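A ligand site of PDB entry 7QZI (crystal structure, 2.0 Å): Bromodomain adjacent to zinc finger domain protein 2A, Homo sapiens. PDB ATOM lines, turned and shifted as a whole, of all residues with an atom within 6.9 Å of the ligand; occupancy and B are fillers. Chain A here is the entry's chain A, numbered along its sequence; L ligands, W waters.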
ATOM      1  N   TRP A  23      -2.549 -12.599  -4.294  1.00  0.00           N
ATOM      2  CA  TRP A  23      -3.258 -11.871  -3.255  1.00  0.00           C
ATOM      3  C   TRP A  23      -4.239 -10.817  -3.767  1.00  0.00           C
ATOM      4  O   TRP A  23      -5.255 -10.621  -3.083  1.00  0.00           O
ATOM      5  CB  TRP A  23      -2.235 -11.239  -2.287  1.00  0.00           C
ATOM      6  CG  TRP A  23      -1.296 -10.251  -2.931  1.00  0.00           C
ATOM      7  CD1 TRP A  23      -0.065 -10.508  -3.463  1.00  0.00           C
ATOM      8  CD2 TRP A  23      -1.521  -8.850  -3.096  1.00  0.00           C
ATOM      9  NE1 TRP A  23       0.492  -9.351  -3.965  1.00  0.00           N
ATOM     10  CE2 TRP A  23      -0.388  -8.319  -3.748  1.00  0.00           C
ATOM     11  CE3 TRP A  23      -2.579  -7.991  -2.760  1.00  0.00           C
ATOM     12  CZ2 TRP A  23      -0.275  -6.964  -4.068  1.00  0.00           C
ATOM     13  CZ3 TRP A  23      -2.466  -6.635  -3.080  1.00  0.00           C
ATOM     14  CH2 TRP A  23      -1.331  -6.142  -3.728  1.00  0.00           C
ATOM     15  N   PRO A  24      -4.061 -10.134  -4.913  1.00  0.00           N
ATOM     16  CA  PRO A  24      -5.111  -9.184  -5.332  1.00  0.00           C
ATOM     17  C   PRO A  24      -6.365  -9.848  -5.868  1.00  0.00           C
ATOM     18  O   PRO A  24      -7.397  -9.185  -5.986  1.00  0.00           O
ATOM     19  CB  PRO A  24      -4.434  -8.349  -6.434  1.00  0.00           C
ATOM     20  CG  PRO A  24      -2.970  -8.728  -6.387  1.00  0.00           C
ATOM     21  CD  PRO A  24      -2.926 -10.109  -5.852  1.00  0.00           C
ATOM     22  N   PHE A  25      -6.297 -11.143  -6.179  1.00  0.00           N
ATOM     23  CA  PHE A  25      -7.316 -11.778  -7.015  1.00  0.00           C
ATOM     24  C   PHE A  25      -8.090 -12.867  -6.289  1.00  0.00           C
ATOM     25  O   PHE A  25      -8.925 -13.543  -6.911  1.00  0.00           O
ATOM     26  CB  PHE A  25      -6.651 -12.347  -8.266  1.00  0.00           C
ATOM     27  CG  PHE A  25      -5.756 -11.352  -8.940  1.00  0.00           C
ATOM     28  CD1 PHE A  25      -6.292 -10.225  -9.574  1.00  0.00           C
ATOM     29  CD2 PHE A  25      -4.373 -11.512  -8.925  1.00  0.00           C
ATOM     30  CE1 PHE A  25      -5.480  -9.294 -10.201  1.00  0.00           C
ATOM     31  CE2 PHE A  25      -3.533 -10.576  -9.540  1.00  0.00           C
ATOM     32  CZ  PHE A  25      -4.080  -9.466 -10.177  1.00  0.00           C
ATOM     33  N   LEU A  26      -7.865 -13.039  -4.990  1.00  0.00           N
ATOM     34  CA  LEU A  26      -8.474 -14.143  -4.269  1.00  0.00           C
ATOM     35  C   LEU A  26      -9.958 -13.902  -3.993  1.00  0.00           C
ATOM     36  O   LEU A  26     -10.714 -14.875  -3.866  1.00  0.00           O
ATOM     37  CB  LEU A  26      -7.731 -14.404  -2.961  1.00  0.00           C
ATOM     38  CG  LEU A  26      -6.273 -14.834  -3.145  1.00  0.00           C
ATOM     39  CD1 LEU A  26      -5.564 -14.938  -1.805  1.00  0.00           C
ATOM     40  CD2 LEU A  26      -6.244 -16.163  -3.868  1.00  0.00           C
ATOM     41  N   GLU A  27     -10.374 -12.650  -3.865  1.00  0.00           N
ATOM     42  CA  GLU A  27     -11.748 -12.284  -3.535  1.00  0.00           C
ATOM     43  C   GLU A  27     -12.217 -11.160  -4.450  1.00  0.00           C
ATOM     44  O   GLU A  27     -11.390 -10.411  -4.961  1.00  0.00           O
ATOM     45  CB  GLU A  27     -11.865 -11.809  -2.072  1.00  0.00           C
ATOM     46  CG  GLU A  27     -11.547 -12.866  -1.022  1.00  0.00           C
ATOM     47  CD  GLU A  27     -12.518 -14.033  -1.065  1.00  0.00           C
ATOM     48  OE1 GLU A  27     -12.052 -15.195  -1.005  1.00  0.00           O
ATOM     49  OE2 GLU A  27     -13.746 -13.802  -1.143  1.00  0.00           O
ATOM     50  N   PRO A  28     -13.533 -11.027  -4.678  1.00  0.00           N
ATOM     51  CA  PRO A  28     -14.024  -9.926  -5.517  1.00  0.00           C
ATOM     52  C   PRO A  28     -13.584  -8.577  -4.964  1.00  0.00           C
ATOM     53  O   PRO A  28     -13.548  -8.372  -3.758  1.00  0.00           O
ATOM     54  CB  PRO A  28     -15.554 -10.080  -5.453  1.00  0.00           C
ATOM     55  CG  PRO A  28     -15.791 -11.493  -5.056  1.00  0.00           C
ATOM     56  CD  PRO A  28     -14.623 -11.886  -4.184  1.00  0.00           C
ATOM     57  N   VAL A  29     -13.249  -7.664  -5.876  1.00  0.00           N
ATOM     58  CA  VAL A  29     -12.963  -6.289  -5.478  1.00  0.00           C
ATOM     59  C   VAL A  29     -14.224  -5.676  -4.863  1.00  0.00           C
ATOM     60  O   VAL A  29     -15.324  -5.842  -5.400  1.00  0.00           O
ATOM     61  CB  VAL A  29     -12.487  -5.489  -6.704  1.00  0.00           C
ATOM     62  CG1 VAL A  29     -12.341  -4.009  -6.367  1.00  0.00           C
ATOM     63  CG2 VAL A  29     -11.150  -6.056  -7.238  1.00  0.00           C
ATOM     64  N   ASN A  30     -14.078  -5.006  -3.725  1.00  0.00           N
ATOM     65  CA  ASN A  30     -15.200  -4.339  -3.087  1.00  0.00           C
ATOM     66  C   ASN A  30     -15.287  -2.929  -3.640  1.00  0.00           C
ATOM     67  O   ASN A  30     -14.425  -2.087  -3.316  1.00  0.00           O
ATOM     68  CB  ASN A  30     -15.040  -4.320  -1.579  1.00  0.00           C
ATOM     69  CG  ASN A  30     -16.294  -3.824  -0.851  1.00  0.00           C
ATOM     70  OD1 ASN A  30     -17.159  -3.157  -1.436  1.00  0.00           O
ATOM     71  ND2 ASN A  30     -16.390  -4.142   0.424  1.00  0.00           N
ATOM     72  N   LEU A  33     -14.766   0.187  -1.525  1.00  0.00           N
ATOM     73  CA  LEU A  33     -13.422   0.517  -1.075  1.00  0.00           C
ATOM     74  C   LEU A  33     -12.539   1.054  -2.192  1.00  0.00           C
ATOM     75  O   LEU A  33     -11.454   1.568  -1.908  1.00  0.00           O
ATOM     76  CB  LEU A  33     -12.755  -0.723  -0.452  1.00  0.00           C
ATOM     77  CG  LEU A  33     -13.553  -1.447   0.631  1.00  0.00           C
ATOM     78  CD1 LEU A  33     -12.787  -2.685   1.107  1.00  0.00           C
ATOM     79  CD2 LEU A  33     -13.841  -0.511   1.800  1.00  0.00           C
ATOM     80  N   VAL A  34     -12.949   0.930  -3.452  1.00  0.00           N
ATOM     81  CA  VAL A  34     -12.091   1.249  -4.583  1.00  0.00           C
ATOM     82  C   VAL A  34     -12.845   2.242  -5.459  1.00  0.00           C
ATOM     83  O   VAL A  34     -13.716   1.852  -6.242  1.00  0.00           O
ATOM     84  CB  VAL A  34     -11.689   0.003  -5.378  1.00  0.00           C
ATOM     85  CG1 VAL A  34     -10.767   0.394  -6.536  1.00  0.00           C
ATOM     86  CG2 VAL A  34     -11.009  -1.000  -4.466  1.00  0.00           C
ATOM     87  N   SER A  35     -12.491   3.518  -5.335  1.00  0.00           N
ATOM     88  CA  SER A  35     -13.174   4.564  -6.079  1.00  0.00           C
ATOM     89  C   SER A  35     -13.025   4.322  -7.575  1.00  0.00           C
ATOM     90  O   SER A  35     -11.922   4.042  -8.066  1.00  0.00           O
ATOM     91  CB  SER A  35     -12.615   5.930  -5.690  1.00  0.00           C
ATOM     92  OG  SER A  35     -13.218   6.955  -6.454  1.00  0.00           O
ATOM     93  N   TYR A  37     -14.100   1.863  -9.454  1.00  0.00           N
ATOM     94  CA  TYR A  37     -13.999   0.503  -9.976  1.00  0.00           C
ATOM     95  C   TYR A  37     -15.285   0.112 -10.685  1.00  0.00           C
ATOM     96  O   TYR A  37     -15.255  -0.418 -11.805  1.00  0.00           O
ATOM     97  CB  TYR A  37     -13.691  -0.480  -8.844  1.00  0.00           C
ATOM     98  CG  TYR A  37     -13.211  -1.809  -9.365  1.00  0.00           C
ATOM     99  CD1 TYR A  37     -11.880  -1.988  -9.740  1.00  0.00           C
ATOM    100  CD2 TYR A  37     -14.081  -2.875  -9.520  1.00  0.00           C
ATOM    101  CE1 TYR A  37     -11.422  -3.200 -10.245  1.00  0.00           C
ATOM    102  CE2 TYR A  37     -13.634  -4.106 -10.018  1.00  0.00           C
ATOM    103  CZ  TYR A  37     -12.306  -4.250 -10.378  1.00  0.00           C
ATOM    104  OH  TYR A  37     -11.838  -5.446 -10.880  1.00  0.00           O
ATOM    105  N   ILE A  41     -14.850  -1.031 -14.621  1.00  0.00           N
ATOM    106  CA  ILE A  41     -14.759  -2.470 -14.862  1.00  0.00           C
ATOM    107  C   ILE A  41     -16.178  -3.010 -15.002  1.00  0.00           C
ATOM    108  O   ILE A  41     -16.898  -3.163 -14.013  1.00  0.00           O
ATOM    109  CB  ILE A  41     -13.978  -3.181 -13.740  1.00  0.00           C
ATOM    110  CG1 ILE A  41     -12.502  -2.789 -13.761  1.00  0.00           C
ATOM    111  CG2 ILE A  41     -14.093  -4.703 -13.880  1.00  0.00           C
ATOM    112  CD1 ILE A  41     -11.808  -3.065 -15.108  1.00  0.00           C
ATOM    113  N   MET A  45     -14.182 -10.116 -12.139  1.00  0.00           N
ATOM    114  CA  MET A  45     -13.931 -11.546 -12.038  1.00  0.00           C
ATOM    115  C   MET A  45     -12.762 -11.727 -11.094  1.00  0.00           C
ATOM    116  O   MET A  45     -11.878 -10.866 -11.030  1.00  0.00           O
ATOM    117  CB  MET A  45     -13.666 -12.172 -13.415  1.00  0.00           C
ATOM    118  CG  MET A  45     -13.489 -13.679 -13.429  1.00  0.00           C
ATOM    119  SD  MET A  45     -14.817 -14.574 -12.586  1.00  0.00           S
ATOM    120  CE  MET A  45     -16.268 -14.011 -13.464  1.00  0.00           C
ATOM    121  N   VAL A  72      -9.883 -11.770 -15.481  1.00  0.00           N
ATOM    122  CA  VAL A  72      -9.212 -11.301 -14.260  1.00  0.00           C
ATOM    123  C   VAL A  72      -8.050 -10.390 -14.621  1.00  0.00           C
ATOM    124  O   VAL A  72      -7.907  -9.284 -14.087  1.00  0.00           O
ATOM    125  CB  VAL A  72      -8.751 -12.494 -13.396  1.00  0.00           C
ATOM    126  CG1 VAL A  72      -7.969 -11.991 -12.205  1.00  0.00           C
ATOM    127  CG2 VAL A  72      -9.959 -13.314 -12.921  1.00  0.00           C
ATOM    128  N   ASN A  75      -9.069  -7.067 -16.589  1.00  0.00           N
ATOM    129  CA  ASN A  75      -9.553  -6.071 -15.632  1.00  0.00           C
ATOM    130  C   ASN A  75      -8.400  -5.460 -14.854  1.00  0.00           C
ATOM    131  O   ASN A  75      -8.369  -4.247 -14.612  1.00  0.00           O
ATOM    132  CB  ASN A  75     -10.545  -6.684 -14.652  1.00  0.00           C
ATOM    133  CG  ASN A  75     -11.829  -7.132 -15.309  1.00  0.00           C
ATOM    134  OD1 ASN A  75     -12.169  -6.680 -16.400  1.00  0.00           O
ATOM    135  ND2 ASN A  75     -12.559  -8.025 -14.643  1.00  0.00           N
ATOM    136  N   CYS A  76      -7.435  -6.298 -14.442  1.00  0.00           N
ATOM    137  CA  CYS A  76      -6.292  -5.821 -13.675  1.00  0.00           C
ATOM    138  C   CYS A  76      -5.519  -4.769 -14.457  1.00  0.00           C
ATOM    139  O   CYS A  76      -5.176  -3.699 -13.930  1.00  0.00           O
ATOM    140  CB  CYS A  76      -5.387  -6.992 -13.315  1.00  0.00           C
ATOM    141  SG  CYS A  76      -3.941  -6.468 -12.366  1.00  0.00           S
ATOM    142  N   PHE A  79      -7.501  -1.401 -14.921  1.00  0.00           N
ATOM    143  CA  PHE A  79      -7.696  -0.501 -13.794  1.00  0.00           C
ATOM    144  C   PHE A  79      -6.407  -0.085 -13.111  1.00  0.00           C
ATOM    145  O   PHE A  79      -6.345   1.020 -12.559  1.00  0.00           O
ATOM    146  CB  PHE A  79      -8.609  -1.160 -12.757  1.00  0.00           C
ATOM    147  CG  PHE A  79      -9.149  -0.186 -11.754  1.00  0.00           C
ATOM    148  CD1 PHE A  79     -10.291   0.560 -12.036  1.00  0.00           C
ATOM    149  CD2 PHE A  79      -8.512   0.013 -10.554  1.00  0.00           C
ATOM    150  CE1 PHE A  79     -10.790   1.455 -11.125  1.00  0.00           C
ATOM    151  CE2 PHE A  79      -8.996   0.932  -9.629  1.00  0.00           C
ATOM    152  CZ  PHE A  79     -10.149   1.638  -9.917  1.00  0.00           C
ATOM    153  N   ASN A  80      -5.372  -0.928 -13.121  1.00  0.00           N
ATOM    154  CA  ASN A  80      -4.159  -0.667 -12.363  1.00  0.00           C
ATOM    155  C   ASN A  80      -2.996  -0.321 -13.274  1.00  0.00           C
ATOM    156  O   ASN A  80      -2.843  -0.922 -14.349  1.00  0.00           O
ATOM    157  CB  ASN A  80      -3.799  -1.891 -11.518  1.00  0.00           C
ATOM    158  CG  ASN A  80      -4.926  -2.294 -10.604  1.00  0.00           C
ATOM    159  OD1 ASN A  80      -5.067  -1.752  -9.507  1.00  0.00           O
ATOM    160  ND2 ASN A  80      -5.754  -3.227 -11.061  1.00  0.00           N
ATOM    161  N   GLU A  85       1.492  -1.982  -7.280  1.00  0.00           N
ATOM    162  CA  GLU A  85       1.687  -3.274  -6.624  1.00  0.00           C
ATOM    163  C   GLU A  85       0.718  -4.320  -7.164  1.00  0.00           C
ATOM    164  O   GLU A  85       1.095  -5.475  -7.381  1.00  0.00           O
ATOM    165  CB  GLU A  85       1.551  -3.151  -5.103  1.00  0.00           C
ATOM    166  CG  GLU A  85       2.752  -2.531  -4.404  1.00  0.00           C
ATOM    167  CD  GLU A  85       4.034  -3.361  -4.523  1.00  0.00           C
ATOM    168  OE1 GLU A  85       3.957  -4.612  -4.520  1.00  0.00           O
ATOM    169  OE2 GLU A  85       5.120  -2.757  -4.620  1.00  0.00           O
ATOM    170  N   VAL A  86      -0.538  -3.930  -7.382  1.00  0.00           N
ATOM    171  CA  VAL A  86      -1.508  -4.878  -7.939  1.00  0.00           C
ATOM    172  C   VAL A  86      -1.191  -5.155  -9.403  1.00  0.00           C
ATOM    173  O   VAL A  86      -1.270  -6.313  -9.862  1.00  0.00           O
ATOM    174  CB  VAL A  86      -2.935  -4.338  -7.747  1.00  0.00           C
ATOM    175  CG1 VAL A  86      -3.932  -5.153  -8.578  1.00  0.00           C
ATOM    176  CG2 VAL A  86      -3.328  -4.350  -6.258  1.00  0.00           C
HETATM  177  C1  LIG L   1      -5.928  -2.117  -5.054  1.00  0.00           C
HETATM  178  C2  LIG L   1      -7.260  -2.865  -4.908  1.00  0.00           C
HETATM  179  C3  LIG L   1      -7.328  -4.258  -5.675  1.00  0.00           C
HETATM  180  C4  LIG L   1      -7.110  -5.506  -5.082  1.00  0.00           C
HETATM  181  C5  LIG L   1      -6.759  -5.840  -3.761  1.00  0.00           C
HETATM  182  C6  LIG L   1      -7.157  -7.067  -3.202  1.00  0.00           C
HETATM  183  C7  LIG L   1      -5.690  -5.542  -1.779  1.00  0.00           C
HETATM  184  C8  LIG L   1      -4.475  -5.478   0.579  1.00  0.00           C
HETATM  185  C9  LIG L   1      -3.438  -4.756   1.459  1.00  0.00           C
HETATM  186  C10 LIG L   1      -2.957  -3.271  -0.395  1.00  0.00           C
HETATM  187  C11 LIG L   1      -4.386  -3.460  -0.959  1.00  0.00           C
HETATM  188  C12 LIG L   1      -5.450  -2.539  -0.280  1.00  0.00           C
HETATM  189  C13 LIG L   1      -6.598  -0.365   0.126  1.00  0.00           C
HETATM  190  C14 LIG L   1      -7.917  -0.171  -0.711  1.00  0.00           C
HETATM  191  C15 LIG L   1      -7.554   0.373  -2.112  1.00  0.00           C
HETATM  192  C16 LIG L   1      -8.664  -1.501  -0.859  1.00  0.00           C
HETATM  193  C17 LIG L   1      -8.829   0.823   0.036  1.00  0.00           C
HETATM  194  C18 LIG L   1      -7.574  -5.932  -7.199  1.00  0.00           C
HETATM  195  C19 LIG L   1      -7.819  -6.761  -8.436  1.00  0.00           C
HETATM  196  C20 LIG L   1      -7.644  -4.547  -7.057  1.00  0.00           C
HETATM  197  C21 LIG L   1      -7.998  -3.602  -8.217  1.00  0.00           C
HETATM  198  C22 LIG L   1      -8.447  -2.142  -7.948  1.00  0.00           C
HETATM  199  N1  LIG L   1      -4.862  -4.851  -0.741  1.00  0.00           N
HETATM  200  N2  LIG L   1      -2.875  -3.514   0.989  1.00  0.00           N
HETATM  201  N3  LIG L   1      -5.552  -1.116  -0.589  1.00  0.00           N
HETATM  202  N4  LIG L   1      -5.983  -5.061  -2.985  1.00  0.00           N
HETATM  203  N5  LIG L   1      -7.261  -6.457  -6.009  1.00  0.00           N
HETATM  204  O1  LIG L   1      -6.226  -3.006   0.467  1.00  0.00           O
HETATM  205  O2  LIG L   1      -7.947  -3.979  -9.343  1.00  0.00           O
HETATM  206  S1  LIG L   1      -6.450  -7.096  -1.608  1.00  0.00           S
HETATM  207  O   HOH W   1      -9.996  -8.716  -3.517  1.00  0.00           O
HETATM  208  O   HOH W   2      -9.038  -5.311 -11.409  1.00  0.00           O
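The backbone carbonyl oxygen (O) of Cys 76 lies within hydrogen-bond range of the side-chain amide nitrogen (ND2) of Asn 80 (3.0 Å).
O of Val 86 sits at hydrogen-bond distance from SG of Cys 76 (3.7 Å).
Water W2 lies within hydrogen-bond range of O2 of the ligand (2.7 Å), OH of Tyr 37 (2.9 Å) and O of Asn 75 (3.4 Å).
The backbone carbonyl oxygen of Pro 24 is in hydrogen-bond range of a nitrogen (N5) of the ligand (2.7 Å).
ND2 of Asn 80 sits at hydrogen-bond distance from O2 of the ligand, at 2.9 Å.
Residues that only touch the ligand: Leu 33 (3.4 Å), Phe 79 (3.4 Å), Val 29 (3.6 Å), Val 86 (3.6 Å), Trp 23 (3.6 Å), Tyr 37 (3.7 Å), Val 34 (3.7 Å) and Phe 25 (3.9 Å).
Within 4 Å of the ligand: Trp 23, Pro 24, Phe 25, Val 29, Leu 33, Val 34, Tyr 37, Phe 79, Asn 80 and Val 86.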
